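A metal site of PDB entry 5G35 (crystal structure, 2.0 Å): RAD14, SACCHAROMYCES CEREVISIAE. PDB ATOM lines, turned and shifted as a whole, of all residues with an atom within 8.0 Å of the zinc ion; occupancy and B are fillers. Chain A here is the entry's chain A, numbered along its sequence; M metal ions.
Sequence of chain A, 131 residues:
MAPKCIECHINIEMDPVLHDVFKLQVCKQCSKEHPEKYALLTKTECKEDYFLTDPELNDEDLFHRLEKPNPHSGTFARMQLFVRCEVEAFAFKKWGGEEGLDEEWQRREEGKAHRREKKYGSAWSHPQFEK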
ATOM      1  N   LYS A   4      30.410   5.148 -27.312  1.00  0.00           N
ATOM      2  CA  LYS A   4      29.093   4.614 -27.699  1.00  0.00           C
ATOM      3  C   LYS A   4      28.824   3.220 -27.179  1.00  0.00           C
ATOM      4  O   LYS A   4      29.752   2.407 -27.039  1.00  0.00           O
ATOM      5  CB  LYS A   4      28.918   4.554 -29.237  1.00  0.00           C
ATOM      6  CG  LYS A   4      29.313   5.814 -30.034  1.00  0.00           C
ATOM      7  CD  LYS A   4      28.406   6.995 -29.763  1.00  0.00           C
ATOM      8  CE  LYS A   4      29.023   8.286 -30.318  1.00  0.00           C
ATOM      9  NZ  LYS A   4      28.484   8.679 -31.625  1.00  0.00           N
ATOM     10  N   CYS A   5      27.534   2.885 -27.032  1.00  0.00           N
ATOM     11  CA  CYS A   5      27.150   1.561 -26.716  1.00  0.00           C
ATOM     12  C   CYS A   5      27.808   0.548 -27.706  1.00  0.00           C
ATOM     13  O   CYS A   5      27.791   0.751 -28.929  1.00  0.00           O
ATOM     14  CB  CYS A   5      25.631   1.452 -26.743  1.00  0.00           C
ATOM     15  SG  CYS A   5      25.063  -0.175 -26.535  1.00  0.00           S
ATOM     16  N   ILE A   6      28.430  -0.512 -27.170  1.00  0.00           N
ATOM     17  CA  ILE A   6      29.001  -1.577 -27.998  1.00  0.00           C
ATOM     18  C   ILE A   6      27.967  -2.405 -28.773  1.00  0.00           C
ATOM     19  O   ILE A   6      28.363  -3.143 -29.657  1.00  0.00           O
ATOM     20  CB  ILE A   6      29.872  -2.568 -27.160  1.00  0.00           C
ATOM     21  CG1 ILE A   6      29.027  -3.272 -26.105  1.00  0.00           C
ATOM     22  CG2 ILE A   6      31.049  -1.841 -26.519  1.00  0.00           C
ATOM     23  CD1 ILE A   6      29.763  -4.304 -25.277  1.00  0.00           C
ATOM     24  N   GLU A   7      26.680  -2.365 -28.451  1.00  0.00           N
ATOM     25  CA  GLU A   7      25.663  -3.097 -29.297  1.00  0.00           C
ATOM     26  C   GLU A   7      25.074  -2.274 -30.384  1.00  0.00           C
ATOM     27  O   GLU A   7      25.066  -2.718 -31.535  1.00  0.00           O
ATOM     28  CB  GLU A   7      24.490  -3.584 -28.485  1.00  0.00           C
ATOM     29  CG  GLU A   7      24.843  -4.650 -27.557  1.00  0.00           C
ATOM     30  CD  GLU A   7      25.043  -6.001 -28.245  1.00  0.00           C
ATOM     31  OE1 GLU A   7      24.528  -6.229 -29.362  1.00  0.00           O
ATOM     32  OE2 GLU A   7      25.711  -6.876 -27.626  1.00  0.00           O
ATOM     33  N   CYS A   8      24.498  -1.102 -30.031  1.00  0.00           N
ATOM     34  CA  CYS A   8      23.842  -0.244 -31.028  1.00  0.00           C
ATOM     35  C   CYS A   8      24.827   0.719 -31.739  1.00  0.00           C
ATOM     36  O   CYS A   8      24.562   1.088 -32.848  1.00  0.00           O
ATOM     37  CB  CYS A   8      22.622   0.541 -30.434  1.00  0.00           C
ATOM     38  SG  CYS A   8      23.039   1.705 -29.126  1.00  0.00           S
ATOM     39  N   HIS A   9      25.918   1.126 -31.094  1.00  0.00           N
ATOM     40  CA  HIS A   9      26.812   2.151 -31.612  1.00  0.00           C
ATOM     41  C   HIS A   9      26.198   3.568 -31.755  1.00  0.00           C
ATOM     42  O   HIS A   9      26.771   4.417 -32.397  1.00  0.00           O
ATOM     43  CB  HIS A   9      27.494   1.703 -32.913  1.00  0.00           C
ATOM     44  CG  HIS A   9      27.935   0.270 -32.884  1.00  0.00           C
ATOM     45  ND1 HIS A   9      29.087  -0.145 -32.223  1.00  0.00           N
ATOM     46  CD2 HIS A   9      27.333  -0.848 -33.333  1.00  0.00           C
ATOM     47  CE1 HIS A   9      29.182  -1.462 -32.314  1.00  0.00           C
ATOM     48  NE2 HIS A   9      28.148  -1.913 -32.998  1.00  0.00           N
ATOM     49  N   ILE A  10      25.133   3.837 -31.025  1.00  0.00           N
ATOM     50  CA  ILE A  10      24.385   5.072 -31.120  1.00  0.00           C
ATOM     51  C   ILE A  10      24.288   5.789 -29.789  1.00  0.00           C
ATOM     52  O   ILE A  10      24.674   6.932 -29.689  1.00  0.00           O
ATOM     53  CB  ILE A  10      23.028   4.742 -31.760  1.00  0.00           C
ATOM     54  CG1 ILE A  10      23.307   4.535 -33.262  1.00  0.00           C
ATOM     55  CG2 ILE A  10      22.022   5.883 -31.601  1.00  0.00           C
ATOM     56  CD1 ILE A  10      22.288   3.681 -33.970  1.00  0.00           C
ATOM     57  N   ASN A  11      23.778   5.075 -28.760  1.00  0.00           N
ATOM     58  CA  ASN A  11      23.513   5.642 -27.461  1.00  0.00           C
ATOM     59  C   ASN A  11      24.851   5.960 -26.774  1.00  0.00           C
ATOM     60  O   ASN A  11      25.876   5.246 -26.940  1.00  0.00           O
ATOM     61  CB  ASN A  11      22.572   4.686 -26.636  1.00  0.00           C
ATOM     62  CG  ASN A  11      21.092   5.072 -26.760  1.00  0.00           C
ATOM     63  OD1 ASN A  11      20.742   6.271 -26.968  1.00  0.00           O
ATOM     64  ND2 ASN A  11      20.207   4.093 -26.566  1.00  0.00           N
ATOM     65  N   ILE A  12      24.870   7.031 -26.008  1.00  0.00           N
ATOM     66  CA  ILE A  12      26.046   7.380 -25.235  1.00  0.00           C
ATOM     67  C   ILE A  12      25.846   7.241 -23.707  1.00  0.00           C
ATOM     68  O   ILE A  12      26.788   7.411 -22.963  1.00  0.00           O
ATOM     69  CB  ILE A  12      26.620   8.766 -25.570  1.00  0.00           C
ATOM     70  CG1 ILE A  12      25.666   9.890 -25.207  1.00  0.00           C
ATOM     71  CG2 ILE A  12      27.013   8.865 -27.034  1.00  0.00           C
ATOM     72  CD1 ILE A  12      26.188  11.235 -25.627  1.00  0.00           C
ATOM     73  N   GLU A  13      24.634   6.921 -23.279  1.00  0.00           N
ATOM     74  CA  GLU A  13      24.316   6.893 -21.908  1.00  0.00           C
ATOM     75  C   GLU A  13      24.132   5.430 -21.637  1.00  0.00           C
ATOM     76  O   GLU A  13      23.204   4.805 -22.156  1.00  0.00           O
ATOM     77  CB  GLU A  13      23.078   7.714 -21.645  1.00  0.00           C
ATOM     78  CG  GLU A  13      23.404   9.185 -21.447  1.00  0.00           C
ATOM     79  CD  GLU A  13      22.649   9.789 -20.240  1.00  0.00           C
ATOM     80  OE1 GLU A  13      22.693   9.213 -19.049  1.00  0.00           O
ATOM     81  OE2 GLU A  13      21.977  10.821 -20.493  1.00  0.00           O
ATOM     82  N   MET A  14      25.011   4.878 -20.824  1.00  0.00           N
ATOM     83  CA  MET A  14      25.015   3.456 -20.579  1.00  0.00           C
ATOM     84  C   MET A  14      24.091   3.073 -19.431  1.00  0.00           C
ATOM     85  O   MET A  14      23.626   3.888 -18.636  1.00  0.00           O
ATOM     86  CB  MET A  14      26.428   2.976 -20.314  1.00  0.00           C
ATOM     87  CG  MET A  14      27.467   3.385 -21.352  1.00  0.00           C
ATOM     88  SD  MET A  14      27.070   2.777 -22.984  1.00  0.00           S
ATOM     89  CE  MET A  14      27.917   4.059 -23.973  1.00  0.00           C
ATOM     90  N   GLN A  25      29.948  -1.615 -21.547  1.00  0.00           N
ATOM     91  CA  GLN A  25      29.541  -0.342 -22.195  1.00  0.00           C
ATOM     92  C   GLN A  25      28.257  -0.511 -23.004  1.00  0.00           C
ATOM     93  O   GLN A  25      28.278  -0.430 -24.255  1.00  0.00           O
ATOM     94  CB  GLN A  25      30.662   0.120 -23.108  1.00  0.00           C
ATOM     95  CG  GLN A  25      31.766   0.885 -22.400  1.00  0.00           C
ATOM     96  CD  GLN A  25      31.320   2.303 -22.125  1.00  0.00           C
ATOM     97  OE1 GLN A  25      30.545   2.878 -22.906  1.00  0.00           O
ATOM     98  NE2 GLN A  25      31.765   2.864 -21.017  1.00  0.00           N
ATOM     99  N   VAL A  26      27.153  -0.800 -22.306  1.00  0.00           N
ATOM    100  CA  VAL A  26      25.858  -1.268 -22.922  1.00  0.00           C
ATOM    101  C   VAL A  26      24.737  -0.360 -22.412  1.00  0.00           C
ATOM    102  O   VAL A  26      24.642  -0.047 -21.191  1.00  0.00           O
ATOM    103  CB  VAL A  26      25.630  -2.762 -22.646  1.00  0.00           C
ATOM    104  CG1 VAL A  26      24.280  -3.313 -23.139  1.00  0.00           C
ATOM    105  CG2 VAL A  26      26.708  -3.525 -23.400  1.00  0.00           C
ATOM    106  N   CYS A  27      23.922   0.067 -23.356  1.00  0.00           N
ATOM    107  CA  CYS A  27      22.799   0.932 -23.043  1.00  0.00           C
ATOM    108  C   CYS A  27      21.638   0.059 -22.536  1.00  0.00           C
ATOM    109  O   CYS A  27      21.609  -1.157 -22.799  1.00  0.00           O
ATOM    110  CB  CYS A  27      22.465   1.833 -24.219  1.00  0.00           C
ATOM    111  SG  CYS A  27      21.434   1.186 -25.517  1.00  0.00           S
ATOM    112  N   LYS A  28      20.729   0.681 -21.790  1.00  0.00           N
ATOM    113  CA  LYS A  28      19.598   0.044 -21.207  1.00  0.00           C
ATOM    114  C   LYS A  28      18.683  -0.532 -22.284  1.00  0.00           C
ATOM    115  O   LYS A  28      18.212  -1.620 -22.162  1.00  0.00           O
ATOM    116  CB  LYS A  28      18.814   1.057 -20.317  1.00  0.00           C
ATOM    117  CG  LYS A  28      17.603   0.391 -19.637  1.00  0.00           C
ATOM    118  CD  LYS A  28      17.265   0.926 -18.220  1.00  0.00           C
ATOM    119  CE  LYS A  28      17.330   2.477 -18.090  1.00  0.00           C
ATOM    120  NZ  LYS A  28      18.657   3.181 -17.802  1.00  0.00           N
ATOM    121  N   GLN A  29      18.400   0.214 -23.359  1.00  0.00           N
ATOM    122  CA  GLN A  29      17.507  -0.364 -24.434  1.00  0.00           C
ATOM    123  C   GLN A  29      18.134  -1.703 -25.021  1.00  0.00           C
ATOM    124  O   GLN A  29      17.457  -2.704 -25.289  1.00  0.00           O
ATOM    125  CB  GLN A  29      17.328   0.671 -25.543  1.00  0.00           C
ATOM    126  CG  GLN A  29      16.463   0.195 -26.696  1.00  0.00           C
ATOM    127  CD  GLN A  29      16.044   1.322 -27.622  1.00  0.00           C
ATOM    128  OE1 GLN A  29      16.573   2.390 -27.594  1.00  0.00           O
ATOM    129  NE2 GLN A  29      15.122   1.031 -28.493  1.00  0.00           N
ATOM    130  N   CYS A  30      19.429  -1.684 -25.193  1.00  0.00           N
ATOM    131  CA  CYS A  30      20.164  -2.794 -25.792  1.00  0.00           C
ATOM    132  C   CYS A  30      20.256  -3.981 -24.822  1.00  0.00           C
ATOM    133  O   CYS A  30      20.136  -5.094 -25.252  1.00  0.00           O
ATOM    134  CB  CYS A  30      21.549  -2.364 -26.234  1.00  0.00           C
ATOM    135  SG  CYS A  30      21.602  -1.368 -27.788  1.00  0.00           S
ATOM    136  N   SER A  31      20.394  -3.707 -23.522  1.00  0.00           N
ATOM    137  CA  SER A  31      20.288  -4.747 -22.568  1.00  0.00           C
ATOM    138  C   SER A  31      18.942  -5.486 -22.689  1.00  0.00           C
ATOM    139  O   SER A  31      18.955  -6.714 -22.705  1.00  0.00           O
ATOM    140  CB  SER A  31      20.616  -4.298 -21.140  1.00  0.00           C
ATOM    141  OG  SER A  31      19.638  -3.525 -20.541  1.00  0.00           O
ATOM    142  N   GLU A  33      16.934  -5.663 -25.301  1.00  0.00           N
ATOM    143  CA  GLU A  33      16.782  -6.299 -26.613  1.00  0.00           C
ATOM    144  C   GLU A  33      17.637  -7.574 -26.721  1.00  0.00           C
ATOM    145  O   GLU A  33      17.434  -8.407 -27.597  1.00  0.00           O
ATOM    146  CB  GLU A  33      17.178  -5.310 -27.741  1.00  0.00           C
ATOM    147  CG  GLU A  33      16.170  -4.175 -27.830  1.00  0.00           C
ATOM    148  CD  GLU A  33      16.495  -2.959 -28.726  1.00  0.00           C
ATOM    149  OE1 GLU A  33      17.651  -2.455 -28.873  1.00  0.00           O
ATOM    150  OE2 GLU A  33      15.477  -2.396 -29.211  1.00  0.00           O
ATOM    151  N   HIS A  34      18.645  -7.717 -25.855  1.00  0.00           N
ATOM    152  CA  HIS A  34      19.579  -8.811 -26.006  1.00  0.00           C
ATOM    153  C   HIS A  34      19.715  -9.489 -24.648  1.00  0.00           C
ATOM    154  O   HIS A  34      20.824  -9.504 -24.108  1.00  0.00           O
ATOM    155  CB  HIS A  34      20.908  -8.275 -26.504  1.00  0.00           C
ATOM    156  CG  HIS A  34      20.829  -7.644 -27.850  1.00  0.00           C
ATOM    157  ND1 HIS A  34      20.846  -8.380 -29.006  1.00  0.00           N
ATOM    158  CD2 HIS A  34      20.677  -6.354 -28.236  1.00  0.00           C
ATOM    159  CE1 HIS A  34      20.698  -7.579 -30.044  1.00  0.00           C
ATOM    160  NE2 HIS A  34      20.618  -6.341 -29.595  1.00  0.00           N
ATOM    161  N   TYR A  38      22.606  -9.990 -21.812  1.00  0.00           N
ATOM    162  CA  TYR A  38      22.618  -9.043 -20.718  1.00  0.00           C
ATOM    163  C   TYR A  38      21.650  -9.337 -19.555  1.00  0.00           C
ATOM    164  O   TYR A  38      21.631  -8.607 -18.605  1.00  0.00           O
ATOM    165  CB  TYR A  38      22.329  -7.699 -21.326  1.00  0.00           C
ATOM    166  CG  TYR A  38      23.401  -7.360 -22.310  1.00  0.00           C
ATOM    167  CD1 TYR A  38      24.725  -7.314 -21.934  1.00  0.00           C
ATOM    168  CD2 TYR A  38      23.083  -7.080 -23.607  1.00  0.00           C
ATOM    169  CE1 TYR A  38      25.705  -7.044 -22.890  1.00  0.00           C
ATOM    170  CE2 TYR A  38      24.064  -6.840 -24.574  1.00  0.00           C
ATOM    171  CZ  TYR A  38      25.363  -6.833 -24.215  1.00  0.00           C
ATOM    172  OH  TYR A  38      26.313  -6.524 -25.193  1.00  0.00           O
HETATM  173 ZN    ZN M   1      22.879   0.305 -27.238  1.00  0.00          ZN
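Four residues have an atom within 4 Å of the zinc ion: Cys 5, Cys 8, Cys 27 and Cys 30. The nearest printed residue that does not touch the zinc ion is Glu 7 (4.4 Å).
The side-chain sulfur (SG) of Cys 5 lies close to the backbone NH (N) of Glu 7 (3.3 Å). N of Cys 5 lies within hydrogen-bond range of O of Asn 11, 2.9 Å away. The side-chain sulfur (SG) of Cys 8 lies close to the backbone NH (N) of Asn 11 (3.5 Å). The side-chain sulfur (SG) of Cys 8 lies close to the backbone NH (N) of Ile 10 (3.5 Å). The side-chain sulfur of Cys 27 sits close to the side-chain amide nitrogen of Asn 11 (3.3 Å).
The zinc ion is bound by the side-chain sulfur (SG) of Cys 30, the side-chain sulfur (SG) of Cys 5, the side-chain sulfur (SG) of Cys 8 and the side-chain sulfur (SG) of Cys 27. The zinc ion has four donor atoms within binding distance.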
